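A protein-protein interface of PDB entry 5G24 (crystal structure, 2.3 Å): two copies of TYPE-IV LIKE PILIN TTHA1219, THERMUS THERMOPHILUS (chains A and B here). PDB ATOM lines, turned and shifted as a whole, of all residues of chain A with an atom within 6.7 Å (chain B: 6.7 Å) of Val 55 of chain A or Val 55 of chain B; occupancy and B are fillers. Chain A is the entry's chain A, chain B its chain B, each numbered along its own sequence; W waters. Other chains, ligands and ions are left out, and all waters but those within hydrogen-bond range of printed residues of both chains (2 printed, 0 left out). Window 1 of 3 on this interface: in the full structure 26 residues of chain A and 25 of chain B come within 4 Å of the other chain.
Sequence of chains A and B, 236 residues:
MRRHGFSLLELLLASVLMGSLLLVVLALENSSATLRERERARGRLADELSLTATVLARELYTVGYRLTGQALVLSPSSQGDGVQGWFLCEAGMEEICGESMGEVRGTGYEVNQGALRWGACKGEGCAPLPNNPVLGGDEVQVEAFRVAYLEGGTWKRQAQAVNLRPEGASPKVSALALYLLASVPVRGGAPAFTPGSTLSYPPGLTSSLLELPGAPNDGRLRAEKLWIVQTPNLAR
The backbone carbonyl oxygen (O) of Val 55 of chain B is in hydrogen-bond range of the guanidinium group (NH1) of Arg 58 of chain A (2.7 Å).
The guanidinium group (NH2) of Arg 58 of chain B is in hydrogen-bond range of the backbone carbonyl oxygen (O) of Arg 58 of chain A.
The side-chain carboxylate (OE1) of Glu 59 of chain B lies within salt-bridge range of the guanidinium group (NH2) of Arg 58 of chain A, at 3.4 Å.
The side-chain carboxylate (OE1) of Glu 59 of chain A is in salt-bridge range of the guanidinium group (NH1) of Arg 58 of chain B, 3.2 Å away.
Among the printed residues, merely in contact across the chains: Leu 51 of chain A with Thr 52 of chain B, Leu 51 of chain A with Val 134 of chain B, Thr 52 of chain A with Leu 51 of chain B, Val 55 of chain A with Val 55 of chain B and Val 134 of chain A with Leu 51 of chain B.
Val 55 of chain A touches just one residue of chain B: Val 55 (3.7 Å).
Val 55 of chain B touches just these residues of chain A: Val 55 and Arg 58.
Of the printed residues of chain B, Val 134 of chain A touches Leu 51 (3.8 Å).
Of the printed residues of chain A, Arg 58 of chain B touches Arg 58 (3.3 Å) and Glu 59 (3.2 Å).
Tyr 109 of chain A touches none of the printed residues of chain B.
Thr 54 of chain B touches none of the printed residues of chain A.
The nearest residue of chain B that does not touch Val 55 of chain A is Leu 51 of chain B (4.1 Å).
The nearest printed residue of chain B that does not touch Val 134 of chain A is Ser 50 of chain B (6.5 Å).
Printed residues of chain A that touch a printed residue of chain B: Leu 51, Thr 52, Val 55, Arg 58, Glu 59 and Val 134.
Of the 13 printed residues of chain B, 6 touch a printed residue of chain A.
Along chain B the printed residues that touch a printed residue of chain A span positions 51 to 134.
Among the printed residues, 9 pairs touch across the chains.
Leu 51 of chain A touches Thr 52 of chain B, and with the chains exchanged Thr 52 of chain A touches Leu 51 of chain B.
Val 55 of chain B touches its own counterpart, Val 55 of chain A.
Arg 58 of chain A touches Val 55 of chain B, but with the chains exchanged Val 55 of chain A does not touch Arg 58 of chain B (4.8 Å).
Arg 58 of chain A touches Glu 59 of chain B, and with the chains exchanged Glu 59 of chain A touches Arg 58 of chain B.
13 positions are printed for both chains.
Of the 9 pairs that touch across the chains among the printed residues, 8 have their exchanged pair printed and touching as well.
Water W1 lies within hydrogen-bond range of the guanidinium group (NH1) of Arg 58 of chain B and the backbone carbonyl oxygen (O) of Val 55 of chain A.
Water W2 lies within hydrogen-bond range of NH2 of Arg 58 of chain A (2.8 Å) and OH of Tyr 109 of chain B (2.9 Å).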
ATOM      1  N   SER A  50      18.287 -20.551   1.749  1.00  0.00           N
ATOM      2  CA  SER A  50      18.318 -20.571   3.201  1.00  0.00           C
ATOM      3  C   SER A  50      19.491 -19.873   3.765  1.00  0.00           C
ATOM      4  O   SER A  50      19.354 -19.095   4.691  1.00  0.00           O
ATOM      5  CB  SER A  50      18.286 -21.992   3.757  1.00  0.00           C
ATOM      6  OG  SER A  50      17.018 -22.509   3.405  1.00  0.00           O
ATOM      7  N   LEU A  51      20.660 -20.156   3.224  1.00  0.00           N
ATOM      8  CA  LEU A  51      21.895 -19.419   3.665  1.00  0.00           C
ATOM      9  C   LEU A  51      21.661 -17.868   3.513  1.00  0.00           C
ATOM     10  O   LEU A  51      22.019 -17.095   4.346  1.00  0.00           O
ATOM     11  CB  LEU A  51      23.121 -19.819   2.856  1.00  0.00           C
ATOM     12  CG  LEU A  51      23.673 -21.176   3.168  1.00  0.00           C
ATOM     13  CD1 LEU A  51      24.613 -21.595   2.033  1.00  0.00           C
ATOM     14  CD2 LEU A  51      24.413 -21.130   4.473  1.00  0.00           C
ATOM     15  N   THR A  52      21.054 -17.514   2.404  1.00  0.00           N
ATOM     16  CA  THR A  52      20.896 -16.118   2.044  1.00  0.00           C
ATOM     17  C   THR A  52      19.987 -15.473   3.044  1.00  0.00           C
ATOM     18  O   THR A  52      20.253 -14.383   3.523  1.00  0.00           O
ATOM     19  CB  THR A  52      20.352 -16.032   0.574  1.00  0.00           C
ATOM     20  OG1 THR A  52      21.366 -16.572  -0.329  1.00  0.00           O
ATOM     21  CG2 THR A  52      20.010 -14.579   0.128  1.00  0.00           C
ATOM     22  N   ALA A  53      18.892 -16.166   3.358  1.00  0.00           N
ATOM     23  CA  ALA A  53      17.901 -15.678   4.307  1.00  0.00           C
ATOM     24  C   ALA A  53      18.536 -15.506   5.676  1.00  0.00           C
ATOM     25  O   ALA A  53      18.210 -14.544   6.418  1.00  0.00           O
ATOM     26  CB  ALA A  53      16.785 -16.652   4.398  1.00  0.00           C
ATOM     27  N   THR A  54      19.461 -16.390   6.050  1.00  0.00           N
ATOM     28  CA  THR A  54      20.104 -16.259   7.359  1.00  0.00           C
ATOM     29  C   THR A  54      20.993 -15.009   7.367  1.00  0.00           C
ATOM     30  O   THR A  54      21.011 -14.283   8.330  1.00  0.00           O
ATOM     31  CB  THR A  54      20.942 -17.462   7.639  1.00  0.00           C
ATOM     32  OG1 THR A  54      20.153 -18.603   7.539  1.00  0.00           O
ATOM     33  CG2 THR A  54      21.597 -17.428   9.034  1.00  0.00           C
ATOM     34  N   VAL A  55      21.740 -14.785   6.286  1.00  0.00           N
ATOM     35  CA  VAL A  55      22.570 -13.611   6.157  1.00  0.00           C
ATOM     36  C   VAL A  55      21.750 -12.317   6.268  1.00  0.00           C
ATOM     37  O   VAL A  55      22.026 -11.463   7.109  1.00  0.00           O
ATOM     38  CB  VAL A  55      23.388 -13.631   4.862  1.00  0.00           C
ATOM     39  CG1 VAL A  55      24.148 -12.313   4.659  1.00  0.00           C
ATOM     40  CG2 VAL A  55      24.411 -14.750   4.902  1.00  0.00           C
ATOM     41  N   LEU A  56      20.688 -12.236   5.488  1.00  0.00           N
ATOM     42  CA  LEU A  56      19.789 -11.093   5.552  1.00  0.00           C
ATOM     43  C   LEU A  56      19.103 -10.924   6.899  1.00  0.00           C
ATOM     44  O   LEU A  56      19.090  -9.817   7.465  1.00  0.00           O
ATOM     45  CB  LEU A  56      18.748 -11.124   4.423  1.00  0.00           C
ATOM     46  CG  LEU A  56      19.207 -10.421   3.185  1.00  0.00           C
ATOM     47  CD1 LEU A  56      20.501 -11.070   2.643  1.00  0.00           C
ATOM     48  CD2 LEU A  56      18.135 -10.448   2.112  1.00  0.00           C
ATOM     49  N   ALA A  57      18.592 -11.995   7.454  1.00  0.00           N
ATOM     50  CA  ALA A  57      17.878 -11.923   8.763  1.00  0.00           C
ATOM     51  C   ALA A  57      18.752 -11.388   9.869  1.00  0.00           C
ATOM     52  O   ALA A  57      18.335 -10.534  10.640  1.00  0.00           O
ATOM     53  CB  ALA A  57      17.288 -13.248   9.181  1.00  0.00           C
ATOM     54  N   ARG A  58      19.947 -11.916   9.980  1.00  0.00           N
ATOM     55  CA  ARG A  58      20.847 -11.455  11.041  1.00  0.00           C
ATOM     56  C   ARG A  58      21.226  -9.995  10.871  1.00  0.00           C
ATOM     57  O   ARG A  58      21.370  -9.288  11.819  1.00  0.00           O
ATOM     58  CB  ARG A  58      22.074 -12.361  11.117  1.00  0.00           C
ATOM     59  CG  ARG A  58      21.759 -13.763  11.642  1.00  0.00           C
ATOM     60  CD  ARG A  58      23.053 -14.540  11.883  1.00  0.00           C
ATOM     61  NE  ARG A  58      22.856 -16.009  12.002  1.00  0.00           N
ATOM     62  CZ  ARG A  58      23.843 -16.905  11.810  1.00  0.00           C
ATOM     63  NH1 ARG A  58      25.113 -16.498  11.461  1.00  0.00           N
ATOM     64  NH2 ARG A  58      23.557 -18.213  11.975  1.00  0.00           N
ATOM     65  N   GLU A  59      21.399  -9.553   9.649  1.00  0.00           N
ATOM     66  CA  GLU A  59      21.676  -8.141   9.338  1.00  0.00           C
ATOM     67  C   GLU A  59      20.442  -7.253   9.685  1.00  0.00           C
ATOM     68  O   GLU A  59      20.527  -6.237  10.396  1.00  0.00           O
ATOM     69  CB  GLU A  59      22.124  -8.052   7.887  1.00  0.00           C
ATOM     70  CG  GLU A  59      22.593  -6.709   7.384  1.00  0.00           C
ATOM     71  CD  GLU A  59      23.993  -6.336   7.738  1.00  0.00           C
ATOM     72  OE1 GLU A  59      24.765  -7.137   8.325  1.00  0.00           O
ATOM     73  OE2 GLU A  59      24.344  -5.192   7.420  1.00  0.00           O
ATOM     74  N   LEU A  60      19.263  -7.667   9.248  1.00  0.00           N
ATOM     75  CA  LEU A  60      18.062  -6.823   9.453  1.00  0.00           C
ATOM     76  C   LEU A  60      17.532  -6.823  10.882  1.00  0.00           C
ATOM     77  O   LEU A  60      16.912  -5.842  11.308  1.00  0.00           O
ATOM     78  CB  LEU A  60      17.003  -7.206   8.450  1.00  0.00           C
ATOM     79  CG  LEU A  60      17.462  -6.912   7.043  1.00  0.00           C
ATOM     80  CD1 LEU A  60      16.595  -7.640   6.041  1.00  0.00           C
ATOM     81  CD2 LEU A  60      17.524  -5.441   6.743  1.00  0.00           C
ATOM     82  N   TYR A 109      19.732  -3.710   0.382  1.00  0.00           N
ATOM     83  CA  TYR A 109      19.591  -4.853  -0.531  1.00  0.00           C
ATOM     84  C   TYR A 109      18.597  -4.550  -1.616  1.00  0.00           C
ATOM     85  O   TYR A 109      17.500  -3.981  -1.367  1.00  0.00           O
ATOM     86  CB  TYR A 109      19.070  -6.080   0.255  1.00  0.00           C
ATOM     87  CG  TYR A 109      19.940  -6.601   1.340  1.00  0.00           C
ATOM     88  CD1 TYR A 109      21.007  -7.428   1.038  1.00  0.00           C
ATOM     89  CD2 TYR A 109      19.719  -6.275   2.672  1.00  0.00           C
ATOM     90  CE1 TYR A 109      21.864  -7.920   2.040  1.00  0.00           C
ATOM     91  CE2 TYR A 109      20.585  -6.764   3.678  1.00  0.00           C
ATOM     92  CZ  TYR A 109      21.616  -7.611   3.359  1.00  0.00           C
ATOM     93  OH  TYR A 109      22.460  -8.137   4.287  1.00  0.00           O
ATOM     94  N   VAL A 134      25.337 -11.153  -3.311  1.00  0.00           N
ATOM     95  CA  VAL A 134      25.114 -12.047  -2.204  1.00  0.00           C
ATOM     96  C   VAL A 134      24.826 -13.411  -2.809  1.00  0.00           C
ATOM     97  O   VAL A 134      25.398 -14.430  -2.432  1.00  0.00           O
ATOM     98  CB  VAL A 134      23.855 -11.575  -1.407  1.00  0.00           C
ATOM     99  CG1 VAL A 134      23.435 -12.549  -0.352  1.00  0.00           C
ATOM    100  CG2 VAL A 134      24.134 -10.232  -0.768  1.00  0.00           C
ATOM    101  N   SER B  50      31.260 -18.627   0.269  1.00  0.00           N
ATOM    102  CA  SER B  50      31.241 -17.300   0.868  1.00  0.00           C
ATOM    103  C   SER B  50      30.047 -17.090   1.759  1.00  0.00           C
ATOM    104  O   SER B  50      30.208 -16.518   2.854  1.00  0.00           O
ATOM    105  CB  SER B  50      31.251 -16.150  -0.195  1.00  0.00           C
ATOM    106  OG  SER B  50      32.527 -16.241  -0.800  1.00  0.00           O
ATOM    107  N   LEU B  51      28.840 -17.396   1.264  1.00  0.00           N
ATOM    108  CA  LEU B  51      27.654 -17.252   2.116  1.00  0.00           C
ATOM    109  C   LEU B  51      27.876 -17.992   3.431  1.00  0.00           C
ATOM    110  O   LEU B  51      27.533 -17.533   4.499  1.00  0.00           O
ATOM    111  CB  LEU B  51      26.422 -17.828   1.483  1.00  0.00           C
ATOM    112  CG  LEU B  51      25.820 -16.980   0.406  1.00  0.00           C
ATOM    113  CD1 LEU B  51      24.864 -17.844  -0.408  1.00  0.00           C
ATOM    114  CD2 LEU B  51      25.091 -15.806   1.046  1.00  0.00           C
ATOM    115  N   THR B  52      28.393 -19.172   3.304  1.00  0.00           N
ATOM    116  CA  THR B  52      28.516 -20.122   4.432  1.00  0.00           C
ATOM    117  C   THR B  52      29.509 -19.537   5.470  1.00  0.00           C
ATOM    118  O   THR B  52      29.203 -19.462   6.603  1.00  0.00           O
ATOM    119  CB  THR B  52      28.949 -21.492   3.899  1.00  0.00           C
ATOM    120  OG1 THR B  52      27.954 -22.038   2.991  1.00  0.00           O
ATOM    121  CG2 THR B  52      29.214 -22.483   5.011  1.00  0.00           C
ATOM    122  N   ALA B  53      30.626 -18.989   4.976  1.00  0.00           N
ATOM    123  CA  ALA B  53      31.621 -18.346   5.742  1.00  0.00           C
ATOM    124  C   ALA B  53      31.040 -17.160   6.476  1.00  0.00           C
ATOM    125  O   ALA B  53      31.406 -16.888   7.631  1.00  0.00           O
ATOM    126  CB  ALA B  53      32.744 -17.896   4.871  1.00  0.00           C
ATOM    127  N   THR B  54      30.156 -16.419   5.840  1.00  0.00           N
ATOM    128  CA  THR B  54      29.603 -15.231   6.476  1.00  0.00           C
ATOM    129  C   THR B  54      28.690 -15.658   7.620  1.00  0.00           C
ATOM    130  O   THR B  54      28.741 -15.089   8.687  1.00  0.00           O
ATOM    131  CB  THR B  54      28.803 -14.410   5.483  1.00  0.00           C
ATOM    132  OG1 THR B  54      29.641 -14.079   4.391  1.00  0.00           O
ATOM    133  CG2 THR B  54      28.213 -13.148   6.096  1.00  0.00           C
ATOM    134  N   VAL B  55      27.899 -16.678   7.401  1.00  0.00           N
ATOM    135  CA  VAL B  55      27.054 -17.212   8.446  1.00  0.00           C
ATOM    136  C   VAL B  55      27.907 -17.673   9.633  1.00  0.00           C
ATOM    137  O   VAL B  55      27.639 -17.282  10.761  1.00  0.00           O
ATOM    138  CB  VAL B  55      26.146 -18.364   7.922  1.00  0.00           C
ATOM    139  CG1 VAL B  55      25.393 -19.036   9.043  1.00  0.00           C
ATOM    140  CG2 VAL B  55      25.139 -17.830   6.869  1.00  0.00           C
ATOM    141  N   LEU B  56      28.900 -18.516   9.383  1.00  0.00           N
ATOM    142  CA  LEU B  56      29.757 -19.014  10.414  1.00  0.00           C
ATOM    143  C   LEU B  56      30.567 -17.894  11.158  1.00  0.00           C
ATOM    144  O   LEU B  56      30.554 -17.832  12.375  1.00  0.00           O
ATOM    145  CB  LEU B  56      30.713 -20.119   9.887  1.00  0.00           C
ATOM    146  CG  LEU B  56      30.187 -21.532  10.007  1.00  0.00           C
ATOM    147  CD1 LEU B  56      28.862 -21.677   9.210  1.00  0.00           C
ATOM    148  CD2 LEU B  56      31.173 -22.536   9.501  1.00  0.00           C
ATOM    149  N   ALA B  57      31.139 -16.952  10.409  1.00  0.00           N
ATOM    150  CA  ALA B  57      31.883 -15.865  10.988  1.00  0.00           C
ATOM    151  C   ALA B  57      31.107 -14.998  11.939  1.00  0.00           C
ATOM    152  O   ALA B  57      31.587 -14.677  13.031  1.00  0.00           O
ATOM    153  CB  ALA B  57      32.511 -14.983   9.918  1.00  0.00           C
ATOM    154  N   ARG B  58      29.916 -14.578  11.518  1.00  0.00           N
ATOM    155  CA  ARG B  58      29.028 -13.770  12.397  1.00  0.00           C
ATOM    156  C   ARG B  58      28.652 -14.496  13.694  1.00  0.00           C
ATOM    157  O   ARG B  58      28.641 -13.911  14.760  1.00  0.00           O
ATOM    158  CB  ARG B  58      27.756 -13.377  11.669  1.00  0.00           C
ATOM    159  CG  ARG B  58      27.151 -12.166  12.315  1.00  0.00           C
ATOM    160  CD  ARG B  58      25.678 -11.923  11.933  1.00  0.00           C
ATOM    161  NE  ARG B  58      25.193 -10.612  12.449  1.00  0.00           N
ATOM    162  CZ  ARG B  58      24.914  -9.526  11.720  1.00  0.00           C
ATOM    163  NH1 ARG B  58      25.040  -9.526  10.374  1.00  0.00           N
ATOM    164  NH2 ARG B  58      24.463  -8.422  12.349  1.00  0.00           N
ATOM    165  N   GLU B  59      28.407 -15.779  13.589  1.00  0.00           N
ATOM    166  CA  GLU B  59      28.091 -16.587  14.741  1.00  0.00           C
ATOM    167  C   GLU B  59      29.345 -16.744  15.692  1.00  0.00           C
ATOM    168  O   GLU B  59      29.300 -16.547  16.916  1.00  0.00           O
ATOM    169  CB  GLU B  59      27.564 -17.921  14.191  1.00  0.00           C
ATOM    170  CG  GLU B  59      26.978 -18.921  15.157  1.00  0.00           C
ATOM    171  CD  GLU B  59      25.553 -18.627  15.608  1.00  0.00           C
ATOM    172  OE1 GLU B  59      24.863 -17.679  15.113  1.00  0.00           O
ATOM    173  OE2 GLU B  59      25.119 -19.367  16.508  1.00  0.00           O
ATOM    174  N   LEU B  60      30.480 -17.065  15.128  1.00  0.00           N
ATOM    175  CA  LEU B  60      31.671 -17.362  15.947  1.00  0.00           C
ATOM    176  C   LEU B  60      32.345 -16.116  16.573  1.00  0.00           C
ATOM    177  O   LEU B  60      32.958 -16.205  17.600  1.00  0.00           O
ATOM    178  CB  LEU B  60      32.654 -18.165  15.125  1.00  0.00           C
ATOM    179  CG  LEU B  60      32.074 -19.524  14.818  1.00  0.00           C
ATOM    180  CD1 LEU B  60      32.926 -20.209  13.734  1.00  0.00           C
ATOM    181  CD2 LEU B  60      31.914 -20.417  16.008  1.00  0.00           C
ATOM    182  N   TYR B 109      29.159 -26.613  14.879  1.00  0.00           N
ATOM    183  CA  TYR B 109      29.286 -27.031  13.475  1.00  0.00           C
ATOM    184  C   TYR B 109      30.204 -28.226  13.295  1.00  0.00           C
ATOM    185  O   TYR B 109      31.286 -28.306  13.940  1.00  0.00           O
ATOM    186  CB  TYR B 109      29.911 -25.897  12.652  1.00  0.00           C
ATOM    187  CG  TYR B 109      29.116 -24.640  12.639  1.00  0.00           C
ATOM    188  CD1 TYR B 109      28.040 -24.522  11.813  1.00  0.00           C
ATOM    189  CD2 TYR B 109      29.425 -23.565  13.512  1.00  0.00           C
ATOM    190  CE1 TYR B 109      27.286 -23.335  11.757  1.00  0.00           C
ATOM    191  CE2 TYR B 109      28.678 -22.384  13.492  1.00  0.00           C
ATOM    192  CZ  TYR B 109      27.600 -22.274  12.571  1.00  0.00           C
ATOM    193  OH  TYR B 109      26.852 -21.132  12.513  1.00  0.00           O
ATOM    194  N   VAL B 134      23.622 -26.866   6.592  1.00  0.00           N
ATOM    195  CA  VAL B 134      23.903 -25.533   6.205  1.00  0.00           C
ATOM    196  C   VAL B 134      24.142 -25.658   4.669  1.00  0.00           C
ATOM    197  O   VAL B 134      23.682 -24.864   3.888  1.00  0.00           O
ATOM    198  CB  VAL B 134      25.193 -25.034   6.958  1.00  0.00           C
ATOM    199  CG1 VAL B 134      25.705 -23.673   6.496  1.00  0.00           C
ATOM    200  CG2 VAL B 134      24.946 -24.946   8.465  1.00  0.00           C
HETATM  201  O   HOH W   1      24.404 -11.565   8.585  1.00  0.00           O
HETATM  202  O   HOH W   2      24.099 -20.956  11.654  1.00  0.00           O
